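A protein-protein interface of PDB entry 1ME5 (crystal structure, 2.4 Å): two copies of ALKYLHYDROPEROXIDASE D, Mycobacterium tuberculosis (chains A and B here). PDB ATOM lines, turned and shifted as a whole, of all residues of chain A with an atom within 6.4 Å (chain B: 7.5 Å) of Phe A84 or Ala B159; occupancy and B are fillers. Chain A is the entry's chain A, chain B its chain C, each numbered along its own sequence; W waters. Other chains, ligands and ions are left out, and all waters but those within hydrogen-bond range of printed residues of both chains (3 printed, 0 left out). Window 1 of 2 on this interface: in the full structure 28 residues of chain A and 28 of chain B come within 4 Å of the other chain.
The guanidinium group (NH2) of Arg A86 sits at hydrogen-bond distance from the backbone carbonyl oxygen (O) of Ala B126 (2.8 Å). NH2 of Arg A86 lies within hydrogen-bond range of O of Ile B127 (3.1 Å).
The side-chain carboxylate (OE2) of Glu B153 lies within salt-bridge range of the side-chain amino group (NZ) of Lys B156 (2.9 Å). O of Ala B158 lies within hydrogen-bond range of OG of Ser B162, at 2.8 Å.
CB of Ser B162 touches O of Gly A79, 3.5 Å away. CA of Met A80 touches O of Ala B159 (3.2 Å). Gly B163 touches Met A80. Ala B126 touches Val A83. Val A83 touches Ser B162 (CG2 to OG, 3.7 Å). Phe A84 touches Phe B152. Leu B155 touches Phe A84. CD2 of Leu B155 touches N of Arg A88 (3.9 Å). CE2 of Phe B152 touches O of Arg A99 (2.9 Å). Ile B160 touches Leu A102 (CD1 to CD2, 3.5 Å).
Of the printed residues of chain B, Val A83 touches Ala B126 (3.3 Å) and Ser B162 (3.7 Å). Of the printed residues of chain B, Arg A88 touches Leu B155. Ala B157 touches none of the printed residues of chain A. Of chain A, only Met A80 and Phe A84 come within 4 Å of Ala B159. Ala B165 touches none of the printed residues of chain A. The nearest residue of chain B that does not touch Phe A84 is Lys B156 (4.3 Å). The nearest printed residue of chain A that does not touch Ser B162 is Met A80 (4.8 Å).
Of the 22 printed residues of chain B, 10 touch a printed residue of chain A. Hydrophobic or aromatic side chains of chain B within 4 Å of the printed part of chain A: Leu B134, Phe B152, Leu B155, Ala B159 and Ile B160. Printed residues of chain A that touch a printed residue of chain B: Gly A79, Met A80, Val A83, Phe A84, Arg A86, Gly A87, Arg A88, Tyr A95, Arg A99, Pro A100 and Leu A102. Among the printed residues, 17 pairs touch across the chains.
No position is printed for both chains.
Water W1 lies within hydrogen-bond range of the backbone carbonyl oxygen of Ala B126 (2.5 Å), the guanidinium group of Arg A86 (2.8 Å), the backbone carbonyl oxygen of Val A83 (2.8 Å) and the backbone NH of Gly A87 (3.2 Å). Water W2 lies within hydrogen-bond range of NZ of Lys B156, O of Arg A99 and O of Pro A100. Water W3 lies within hydrogen-bond range of the backbone carbonyl oxygen (O) of Gly A101 (2.8 Å) and the side-chain amino group (NZ) of Lys B156 (3.1 Å).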
ATOM      1  N   GLY A  79     -28.876 -13.338  -0.725  1.00  0.00           N
ATOM      2  CA  GLY A  79     -29.137 -14.345   0.287  1.00  0.00           C
ATOM      3  C   GLY A  79     -29.249 -15.731  -0.323  1.00  0.00           C
ATOM      4  O   GLY A  79     -28.883 -16.714   0.312  1.00  0.00           O
ATOM      5  N   MET A  80     -29.782 -15.821  -1.546  1.00  0.00           N
ATOM      6  CA  MET A  80     -29.888 -17.110  -2.229  1.00  0.00           C
ATOM      7  C   MET A  80     -28.540 -17.449  -2.870  1.00  0.00           C
ATOM      8  O   MET A  80     -27.965 -18.513  -2.641  1.00  0.00           O
ATOM      9  CB  MET A  80     -30.964 -17.069  -3.326  1.00  0.00           C
ATOM     10  CG  MET A  80     -30.858 -18.217  -4.345  1.00  0.00           C
ATOM     11  SD  MET A  80     -32.214 -18.186  -5.611  1.00  0.00           S
ATOM     12  CE  MET A  80     -31.707 -16.768  -6.525  1.00  0.00           C
ATOM     13  N   ASN A  81     -28.047 -16.515  -3.673  1.00  0.00           N
ATOM     14  CA  ASN A  81     -26.796 -16.694  -4.368  1.00  0.00           C
ATOM     15  C   ASN A  81     -25.539 -16.884  -3.511  1.00  0.00           C
ATOM     16  O   ASN A  81     -24.697 -17.703  -3.850  1.00  0.00           O
ATOM     17  CB  ASN A  81     -26.603 -15.550  -5.354  1.00  0.00           C
ATOM     18  CG  ASN A  81     -27.484 -15.702  -6.565  1.00  0.00           C
ATOM     19  OD1 ASN A  81     -28.053 -16.784  -6.800  1.00  0.00           O
ATOM     20  ND2 ASN A  81     -27.603 -14.633  -7.353  1.00  0.00           N
ATOM     21  N   ASN A  82     -25.396 -16.149  -2.414  1.00  0.00           N
ATOM     22  CA  ASN A  82     -24.203 -16.322  -1.578  1.00  0.00           C
ATOM     23  C   ASN A  82     -24.082 -17.761  -1.089  1.00  0.00           C
ATOM     24  O   ASN A  82     -22.978 -18.268  -0.923  1.00  0.00           O
ATOM     25  CB  ASN A  82     -24.239 -15.387  -0.371  1.00  0.00           C
ATOM     26  CG  ASN A  82     -24.239 -13.940  -0.762  1.00  0.00           C
ATOM     27  OD1 ASN A  82     -24.788 -13.106  -0.049  1.00  0.00           O
ATOM     28  ND2 ASN A  82     -23.627 -13.624  -1.907  1.00  0.00           N
ATOM     29  N   VAL A  83     -25.215 -18.421  -0.868  1.00  0.00           N
ATOM     30  CA  VAL A  83     -25.169 -19.788  -0.405  1.00  0.00           C
ATOM     31  C   VAL A  83     -24.879 -20.762  -1.527  1.00  0.00           C
ATOM     32  O   VAL A  83     -23.991 -21.605  -1.393  1.00  0.00           O
ATOM     33  CB  VAL A  83     -26.475 -20.227   0.293  1.00  0.00           C
ATOM     34  CG1 VAL A  83     -26.363 -21.685   0.692  1.00  0.00           C
ATOM     35  CG2 VAL A  83     -26.718 -19.381   1.518  1.00  0.00           C
ATOM     36  N   PHE A  84     -25.628 -20.670  -2.620  1.00  0.00           N
ATOM     37  CA  PHE A  84     -25.416 -21.572  -3.745  1.00  0.00           C
ATOM     38  C   PHE A  84     -23.994 -21.543  -4.237  1.00  0.00           C
ATOM     39  O   PHE A  84     -23.309 -22.553  -4.194  1.00  0.00           O
ATOM     40  CB  PHE A  84     -26.317 -21.238  -4.927  1.00  0.00           C
ATOM     41  CG  PHE A  84     -26.038 -22.077  -6.147  1.00  0.00           C
ATOM     42  CD1 PHE A  84     -26.526 -23.371  -6.243  1.00  0.00           C
ATOM     43  CD2 PHE A  84     -25.265 -21.572  -7.199  1.00  0.00           C
ATOM     44  CE1 PHE A  84     -26.258 -24.157  -7.362  1.00  0.00           C
ATOM     45  CE2 PHE A  84     -24.987 -22.350  -8.327  1.00  0.00           C
ATOM     46  CZ  PHE A  84     -25.486 -23.642  -8.409  1.00  0.00           C
ATOM     47  N   TYR A  85     -23.546 -20.386  -4.708  1.00  0.00           N
ATOM     48  CA  TYR A  85     -22.193 -20.255  -5.231  1.00  0.00           C
ATOM     49  C   TYR A  85     -21.104 -20.680  -4.262  1.00  0.00           C
ATOM     50  O   TYR A  85     -20.126 -21.285  -4.677  1.00  0.00           O
ATOM     51  CB  TYR A  85     -21.953 -18.821  -5.723  1.00  0.00           C
ATOM     52  CG  TYR A  85     -22.845 -18.470  -6.903  1.00  0.00           C
ATOM     53  CD1 TYR A  85     -22.697 -19.115  -8.133  1.00  0.00           C
ATOM     54  CD2 TYR A  85     -23.892 -17.562  -6.763  1.00  0.00           C
ATOM     55  CE1 TYR A  85     -23.574 -18.867  -9.186  1.00  0.00           C
ATOM     56  CE2 TYR A  85     -24.768 -17.308  -7.805  1.00  0.00           C
ATOM     57  CZ  TYR A  85     -24.606 -17.961  -9.011  1.00  0.00           C
ATOM     58  OH  TYR A  85     -25.483 -17.701 -10.029  1.00  0.00           O
ATOM     59  N   ARG A  86     -21.266 -20.372  -2.977  1.00  0.00           N
ATOM     60  CA  ARG A  86     -20.261 -20.752  -1.980  1.00  0.00           C
ATOM     61  C   ARG A  86     -20.206 -22.280  -1.895  1.00  0.00           C
ATOM     62  O   ARG A  86     -19.136 -22.872  -1.956  1.00  0.00           O
ATOM     63  CB  ARG A  86     -20.613 -20.149  -0.607  1.00  0.00           C
ATOM     64  CG  ARG A  86     -19.504 -20.226   0.429  1.00  0.00           C
ATOM     65  CD  ARG A  86     -19.918 -19.556   1.744  1.00  0.00           C
ATOM     66  NE  ARG A  86     -21.007 -20.280   2.384  1.00  0.00           N
ATOM     67  CZ  ARG A  86     -21.708 -19.831   3.418  1.00  0.00           C
ATOM     68  NH1 ARG A  86     -21.430 -18.650   3.945  1.00  0.00           N
ATOM     69  NH2 ARG A  86     -22.709 -20.553   3.908  1.00  0.00           N
ATOM     70  N   GLY A  87     -21.372 -22.915  -1.778  1.00  0.00           N
ATOM     71  CA  GLY A  87     -21.430 -24.364  -1.697  1.00  0.00           C
ATOM     72  C   GLY A  87     -20.787 -25.049  -2.892  1.00  0.00           C
ATOM     73  O   GLY A  87     -20.035 -26.007  -2.729  1.00  0.00           O
ATOM     74  N   ARG A  88     -21.095 -24.552  -4.088  1.00  0.00           N
ATOM     75  CA  ARG A  88     -20.574 -25.092  -5.330  1.00  0.00           C
ATOM     76  C   ARG A  88     -19.056 -24.950  -5.390  1.00  0.00           C
ATOM     77  O   ARG A  88     -18.369 -25.797  -5.963  1.00  0.00           O
ATOM     78  CB  ARG A  88     -21.224 -24.380  -6.527  1.00  0.00           C
ATOM     79  CG  ARG A  88     -21.593 -25.317  -7.674  1.00  0.00           C
ATOM     80  CD  ARG A  88     -22.253 -24.588  -8.834  1.00  0.00           C
ATOM     81  NE  ARG A  88     -21.457 -23.453  -9.278  1.00  0.00           N
ATOM     82  CZ  ARG A  88     -21.714 -22.736 -10.366  1.00  0.00           C
ATOM     83  NH1 ARG A  88     -22.754 -23.044 -11.132  1.00  0.00           N
ATOM     84  NH2 ARG A  88     -20.940 -21.699 -10.674  1.00  0.00           N
ATOM     85  N   GLY A  89     -18.531 -23.883  -4.793  1.00  0.00           N
ATOM     86  CA  GLY A  89     -17.094 -23.678  -4.778  1.00  0.00           C
ATOM     87  C   GLY A  89     -16.421 -24.638  -3.819  1.00  0.00           C
ATOM     88  O   GLY A  89     -15.264 -25.011  -4.003  1.00  0.00           O
ATOM     89  N   TYR A  95     -19.237 -29.508  -9.857  1.00  0.00           N
ATOM     90  CA  TYR A  95     -20.620 -29.279 -10.236  1.00  0.00           C
ATOM     91  C   TYR A  95     -20.711 -27.970 -11.008  1.00  0.00           C
ATOM     92  O   TYR A  95     -21.787 -27.583 -11.441  1.00  0.00           O
ATOM     93  CB  TYR A  95     -21.501 -29.145  -8.988  1.00  0.00           C
ATOM     94  CG  TYR A  95     -21.825 -30.409  -8.229  1.00  0.00           C
ATOM     95  CD1 TYR A  95     -20.870 -31.042  -7.435  1.00  0.00           C
ATOM     96  CD2 TYR A  95     -23.110 -30.954  -8.276  1.00  0.00           C
ATOM     97  CE1 TYR A  95     -21.198 -32.198  -6.691  1.00  0.00           C
ATOM     98  CE2 TYR A  95     -23.441 -32.103  -7.548  1.00  0.00           C
ATOM     99  CZ  TYR A  95     -22.487 -32.715  -6.758  1.00  0.00           C
ATOM    100  OH  TYR A  95     -22.821 -33.833  -6.028  1.00  0.00           O
ATOM    101  N   ARG A  99     -25.825 -26.761 -14.082  1.00  0.00           N
ATOM    102  CA  ARG A  99     -26.925 -25.831 -14.332  1.00  0.00           C
ATOM    103  C   ARG A  99     -27.751 -25.466 -13.093  1.00  0.00           C
ATOM    104  O   ARG A  99     -28.616 -26.232 -12.655  1.00  0.00           O
ATOM    105  CB  ARG A  99     -27.859 -26.375 -15.416  1.00  0.00           C
ATOM    106  CG  ARG A  99     -28.992 -25.434 -15.772  1.00  0.00           C
ATOM    107  CD  ARG A  99     -29.708 -25.884 -17.029  1.00  0.00           C
ATOM    108  NE  ARG A  99     -30.544 -27.063 -16.816  1.00  0.00           N
ATOM    109  CZ  ARG A  99     -31.065 -27.792 -17.799  1.00  0.00           C
ATOM    110  NH1 ARG A  99     -30.831 -27.467 -19.065  1.00  0.00           N
ATOM    111  NH2 ARG A  99     -31.828 -28.839 -17.518  1.00  0.00           N
ATOM    112  N   PRO A 100     -27.502 -24.274 -12.528  1.00  0.00           N
ATOM    113  CA  PRO A 100     -28.218 -23.800 -11.342  1.00  0.00           C
ATOM    114  C   PRO A 100     -29.735 -23.710 -11.504  1.00  0.00           C
ATOM    115  O   PRO A 100     -30.477 -24.139 -10.622  1.00  0.00           O
ATOM    116  CB  PRO A 100     -27.570 -22.442 -11.063  1.00  0.00           C
ATOM    117  CG  PRO A 100     -27.087 -22.011 -12.408  1.00  0.00           C
ATOM    118  CD  PRO A 100     -26.519 -23.277 -12.975  1.00  0.00           C
ATOM    119  N   GLY A 101     -30.186 -23.155 -12.627  1.00  0.00           N
ATOM    120  CA  GLY A 101     -31.612 -23.027 -12.872  1.00  0.00           C
ATOM    121  C   GLY A 101     -32.291 -22.219 -11.783  1.00  0.00           C
ATOM    122  O   GLY A 101     -33.386 -22.556 -11.328  1.00  0.00           O
ATOM    123  N   LEU A 102     -31.619 -21.151 -11.359  1.00  0.00           N
ATOM    124  CA  LEU A 102     -32.119 -20.259 -10.320  1.00  0.00           C
ATOM    125  C   LEU A 102     -32.311 -18.882 -10.925  1.00  0.00           C
ATOM    126  O   LEU A 102     -31.358 -18.266 -11.400  1.00  0.00           O
ATOM    127  CB  LEU A 102     -31.117 -20.170  -9.173  1.00  0.00           C
ATOM    128  CG  LEU A 102     -30.794 -21.453  -8.414  1.00  0.00           C
ATOM    129  CD1 LEU A 102     -29.787 -21.125  -7.312  1.00  0.00           C
ATOM    130  CD2 LEU A 102     -32.058 -22.038  -7.820  1.00  0.00           C
ATOM    131  N   ILE B  17     -37.018 -14.937  -6.077  1.00  0.00           N
ATOM    132  CA  ILE B  17     -37.059 -15.847  -4.927  1.00  0.00           C
ATOM    133  C   ILE B  17     -38.423 -16.557  -4.867  1.00  0.00           C
ATOM    134  O   ILE B  17     -38.510 -17.755  -4.577  1.00  0.00           O
ATOM    135  CB  ILE B  17     -36.789 -15.055  -3.608  1.00  0.00           C
ATOM    136  CG1 ILE B  17     -35.348 -14.542  -3.621  1.00  0.00           C
ATOM    137  CG2 ILE B  17     -37.049 -15.923  -2.380  1.00  0.00           C
ATOM    138  CD1 ILE B  17     -35.064 -13.508  -2.580  1.00  0.00           C
ATOM    139  N   THR B  38     -35.454 -31.496   3.252  1.00  0.00           N
ATOM    140  CA  THR B  38     -34.364 -30.539   3.088  1.00  0.00           C
ATOM    141  C   THR B  38     -34.909 -29.147   3.336  1.00  0.00           C
ATOM    142  O   THR B  38     -34.296 -28.350   4.044  1.00  0.00           O
ATOM    143  CB  THR B  38     -33.747 -30.598   1.672  1.00  0.00           C
ATOM    144  OG1 THR B  38     -33.067 -31.840   1.515  1.00  0.00           O
ATOM    145  CG2 THR B  38     -32.744 -29.467   1.469  1.00  0.00           C
ATOM    146  N   SER B  42     -33.186 -26.724   6.091  1.00  0.00           N
ATOM    147  CA  SER B  42     -32.625 -25.456   5.652  1.00  0.00           C
ATOM    148  C   SER B  42     -33.274 -24.278   6.389  1.00  0.00           C
ATOM    149  O   SER B  42     -32.592 -23.362   6.855  1.00  0.00           O
ATOM    150  CB  SER B  42     -32.837 -25.296   4.141  1.00  0.00           C
ATOM    151  OG  SER B  42     -32.083 -26.243   3.399  1.00  0.00           O
ATOM    152  N   THR B  46     -31.889 -21.107   8.838  1.00  0.00           N
ATOM    153  CA  THR B  46     -31.864 -19.688   8.480  1.00  0.00           C
ATOM    154  C   THR B  46     -32.113 -18.848   9.722  1.00  0.00           C
ATOM    155  O   THR B  46     -31.753 -17.675   9.775  1.00  0.00           O
ATOM    156  CB  THR B  46     -32.934 -19.335   7.434  1.00  0.00           C
ATOM    157  OG1 THR B  46     -34.233 -19.642   7.951  1.00  0.00           O
ATOM    158  CG2 THR B  46     -32.695 -20.123   6.134  1.00  0.00           C
ATOM    159  N   ALA B 123     -27.477 -29.777   2.918  1.00  0.00           N
ATOM    160  CA  ALA B 123     -28.244 -28.553   2.882  1.00  0.00           C
ATOM    161  C   ALA B 123     -27.872 -27.550   3.977  1.00  0.00           C
ATOM    162  O   ALA B 123     -27.590 -26.388   3.680  1.00  0.00           O
ATOM    163  CB  ALA B 123     -29.710 -28.902   2.982  1.00  0.00           C
ATOM    164  N   ALA B 126     -24.421 -26.152   3.784  1.00  0.00           N
ATOM    165  CA  ALA B 126     -24.352 -25.172   2.700  1.00  0.00           C
ATOM    166  C   ALA B 126     -24.739 -23.802   3.233  1.00  0.00           C
ATOM    167  O   ALA B 126     -24.110 -22.791   2.895  1.00  0.00           O
ATOM    168  CB  ALA B 126     -25.295 -25.572   1.536  1.00  0.00           C
ATOM    169  N   ILE B 127     -25.777 -23.779   4.065  1.00  0.00           N
ATOM    170  CA  ILE B 127     -26.275 -22.536   4.652  1.00  0.00           C
ATOM    171  C   ILE B 127     -25.347 -21.952   5.728  1.00  0.00           C
ATOM    172  O   ILE B 127     -25.135 -20.737   5.778  1.00  0.00           O
ATOM    173  CB  ILE B 127     -27.711 -22.736   5.234  1.00  0.00           C
ATOM    174  CG1 ILE B 127     -28.714 -22.860   4.075  1.00  0.00           C
ATOM    175  CG2 ILE B 127     -28.074 -21.585   6.151  1.00  0.00           C
ATOM    176  CD1 ILE B 127     -30.093 -23.382   4.450  1.00  0.00           C
ATOM    177  N   LEU B 134     -19.648 -29.901   4.264  1.00  0.00           N
ATOM    178  CA  LEU B 134     -20.376 -29.955   3.008  1.00  0.00           C
ATOM    179  C   LEU B 134     -19.800 -31.081   2.142  1.00  0.00           C
ATOM    180  O   LEU B 134     -20.539 -31.855   1.533  1.00  0.00           O
ATOM    181  CB  LEU B 134     -20.257 -28.630   2.256  1.00  0.00           C
ATOM    182  CG  LEU B 134     -21.137 -28.567   1.007  1.00  0.00           C
ATOM    183  CD1 LEU B 134     -22.570 -28.520   1.475  1.00  0.00           C
ATOM    184  CD2 LEU B 134     -20.816 -27.350   0.144  1.00  0.00           C
ATOM    185  N   PHE B 152     -27.432 -31.737  -5.938  1.00  0.00           N
ATOM    186  CA  PHE B 152     -27.365 -30.379  -6.447  1.00  0.00           C
ATOM    187  C   PHE B 152     -28.652 -29.649  -6.112  1.00  0.00           C
ATOM    188  O   PHE B 152     -28.626 -28.519  -5.622  1.00  0.00           O
ATOM    189  CB  PHE B 152     -27.192 -30.427  -7.958  1.00  0.00           C
ATOM    190  CG  PHE B 152     -26.997 -29.090  -8.600  1.00  0.00           C
ATOM    191  CD1 PHE B 152     -25.896 -28.307  -8.280  1.00  0.00           C
ATOM    192  CD2 PHE B 152     -27.864 -28.655  -9.591  1.00  0.00           C
ATOM    193  CE1 PHE B 152     -25.656 -27.111  -8.951  1.00  0.00           C
ATOM    194  CE2 PHE B 152     -27.633 -27.456 -10.271  1.00  0.00           C
ATOM    195  CZ  PHE B 152     -26.525 -26.685  -9.951  1.00  0.00           C
ATOM    196  N   GLU B 153     -29.778 -30.303  -6.399  1.00  0.00           N
ATOM    197  CA  GLU B 153     -31.109 -29.751  -6.139  1.00  0.00           C
ATOM    198  C   GLU B 153     -31.233 -29.389  -4.660  1.00  0.00           C
ATOM    199  O   GLU B 153     -31.842 -28.396  -4.311  1.00  0.00           O
ATOM    200  CB  GLU B 153     -32.200 -30.769  -6.512  1.00  0.00           C
ATOM    201  CG  GLU B 153     -33.579 -30.176  -6.721  1.00  0.00           C
ATOM    202  CD  GLU B 153     -33.721 -29.480  -8.072  1.00  0.00           C
ATOM    203  OE1 GLU B 153     -34.840 -29.013  -8.404  1.00  0.00           O
ATOM    204  OE2 GLU B 153     -32.713 -29.399  -8.807  1.00  0.00           O
ATOM    205  N   ALA B 154     -30.648 -30.201  -3.797  1.00  0.00           N
ATOM    206  CA  ALA B 154     -30.700 -29.933  -2.371  1.00  0.00           C
ATOM    207  C   ALA B 154     -29.959 -28.632  -2.047  1.00  0.00           C
ATOM    208  O   ALA B 154     -30.418 -27.852  -1.219  1.00  0.00           O
ATOM    209  CB  ALA B 154     -30.098 -31.113  -1.589  1.00  0.00           C
ATOM    210  N   LEU B 155     -28.813 -28.411  -2.699  1.00  0.00           N
ATOM    211  CA  LEU B 155     -28.014 -27.193  -2.494  1.00  0.00           C
ATOM    212  C   LEU B 155     -28.888 -26.041  -2.960  1.00  0.00           C
ATOM    213  O   LEU B 155     -28.948 -24.995  -2.313  1.00  0.00           O
ATOM    214  CB  LEU B 155     -26.700 -27.248  -3.306  1.00  0.00           C
ATOM    215  CG  LEU B 155     -25.800 -26.000  -3.455  1.00  0.00           C
ATOM    216  CD1 LEU B 155     -25.399 -25.445  -2.092  1.00  0.00           C
ATOM    217  CD2 LEU B 155     -24.540 -26.363  -4.251  1.00  0.00           C
ATOM    218  N   LYS B 156     -29.583 -26.270  -4.076  1.00  0.00           N
ATOM    219  CA  LYS B 156     -30.505 -25.300  -4.658  1.00  0.00           C
ATOM    220  C   LYS B 156     -31.613 -25.015  -3.651  1.00  0.00           C
ATOM    221  O   LYS B 156     -32.056 -23.873  -3.502  1.00  0.00           O
ATOM    222  CB  LYS B 156     -31.127 -25.854  -5.944  1.00  0.00           C
ATOM    223  CG  LYS B 156     -30.150 -26.039  -7.090  1.00  0.00           C
ATOM    224  CD  LYS B 156     -30.826 -26.721  -8.248  1.00  0.00           C
ATOM    225  CE  LYS B 156     -32.052 -25.939  -8.711  1.00  0.00           C
ATOM    226  NZ  LYS B 156     -32.815 -26.642  -9.784  1.00  0.00           N
ATOM    227  N   ALA B 157     -32.061 -26.071  -2.973  1.00  0.00           N
ATOM    228  CA  ALA B 157     -33.096 -25.966  -1.955  1.00  0.00           C
ATOM    229  C   ALA B 157     -32.585 -25.105  -0.781  1.00  0.00           C
ATOM    230  O   ALA B 157     -33.247 -24.166  -0.364  1.00  0.00           O
ATOM    231  CB  ALA B 157     -33.502 -27.369  -1.457  1.00  0.00           C
ATOM    232  N   ALA B 158     -31.409 -25.426  -0.260  1.00  0.00           N
ATOM    233  CA  ALA B 158     -30.839 -24.657   0.848  1.00  0.00           C
ATOM    234  C   ALA B 158     -30.697 -23.189   0.441  1.00  0.00           C
ATOM    235  O   ALA B 158     -31.072 -22.279   1.193  1.00  0.00           O
ATOM    236  CB  ALA B 158     -29.483 -25.228   1.244  1.00  0.00           C
ATOM    237  N   ALA B 159     -30.182 -22.966  -0.762  1.00  0.00           N
ATOM    238  CA  ALA B 159     -29.998 -21.619  -1.271  1.00  0.00           C
ATOM    239  C   ALA B 159     -31.305 -20.871  -1.419  1.00  0.00           C
ATOM    240  O   ALA B 159     -31.374 -19.703  -1.080  1.00  0.00           O
ATOM    241  CB  ALA B 159     -29.271 -21.651  -2.615  1.00  0.00           C
ATOM    242  N   ILE B 160     -32.344 -21.529  -1.931  1.00  0.00           N
ATOM    243  CA  ILE B 160     -33.619 -20.845  -2.106  1.00  0.00           C
ATOM    244  C   ILE B 160     -34.322 -20.576  -0.769  1.00  0.00           C
ATOM    245  O   ILE B 160     -34.944 -19.530  -0.593  1.00  0.00           O
ATOM    246  CB  ILE B 160     -34.550 -21.614  -3.083  1.00  0.00           C
ATOM    247  CG1 ILE B 160     -33.871 -21.703  -4.443  1.00  0.00           C
ATOM    248  CG2 ILE B 160     -35.868 -20.854  -3.274  1.00  0.00           C
ATOM    249  CD1 ILE B 160     -34.541 -22.629  -5.411  1.00  0.00           C
ATOM    250  N   VAL B 161     -34.218 -21.515   0.167  1.00  0.00           N
ATOM    251  CA  VAL B 161     -34.808 -21.326   1.494  1.00  0.00           C
ATOM    252  C   VAL B 161     -34.144 -20.094   2.144  1.00  0.00           C
ATOM    253  O   VAL B 161     -34.815 -19.264   2.767  1.00  0.00           O
ATOM    254  CB  VAL B 161     -34.570 -22.551   2.427  1.00  0.00           C
ATOM    255  CG1 VAL B 161     -35.134 -22.266   3.800  1.00  0.00           C
ATOM    256  CG2 VAL B 161     -35.230 -23.807   1.855  1.00  0.00           C
ATOM    257  N   SER B 162     -32.826 -19.977   1.968  1.00  0.00           N
ATOM    258  CA  SER B 162     -32.075 -18.861   2.541  1.00  0.00           C
ATOM    259  C   SER B 162     -32.537 -17.523   1.960  1.00  0.00           C
ATOM    260  O   SER B 162     -32.585 -16.514   2.665  1.00  0.00           O
ATOM    261  CB  SER B 162     -30.566 -19.040   2.295  1.00  0.00           C
ATOM    262  OG  SER B 162     -30.057 -20.253   2.848  1.00  0.00           O
ATOM    263  N   GLY B 163     -32.868 -17.534   0.665  1.00  0.00           N
ATOM    264  CA  GLY B 163     -33.321 -16.344  -0.028  1.00  0.00           C
ATOM    265  C   GLY B 163     -34.673 -15.901   0.484  1.00  0.00           C
ATOM    266  O   GLY B 163     -34.901 -14.707   0.680  1.00  0.00           O
ATOM    267  N   VAL B 164     -35.570 -16.866   0.695  1.00  0.00           N
ATOM    268  CA  VAL B 164     -36.903 -16.592   1.236  1.00  0.00           C
ATOM    269  C   VAL B 164     -36.756 -15.936   2.623  1.00  0.00           C
ATOM    270  O   VAL B 164     -37.357 -14.899   2.895  1.00  0.00           O
ATOM    271  CB  VAL B 164     -37.740 -17.893   1.419  1.00  0.00           C
ATOM    272  CG1 VAL B 164     -39.094 -17.538   2.030  1.00  0.00           C
ATOM    273  CG2 VAL B 164     -37.936 -18.612   0.074  1.00  0.00           C
ATOM    274  N   ALA B 165     -35.957 -16.552   3.491  1.00  0.00           N
ATOM    275  CA  ALA B 165     -35.722 -16.020   4.834  1.00  0.00           C
ATOM    276  C   ALA B 165     -35.301 -14.547   4.767  1.00  0.00           C
ATOM    277  O   ALA B 165     -35.895 -13.692   5.413  1.00  0.00           O
ATOM    278  CB  ALA B 165     -34.654 -16.842   5.549  1.00  0.00           C
HETATM  279  O   HOH W   1     -22.663 -22.071   1.030  1.00  0.00           O
HETATM  280  O   HOH W   2     -31.225 -27.161 -12.038  1.00  0.00           O
HETATM  281  O   HOH W   3     -35.076 -24.700 -10.643  1.00  0.00           O
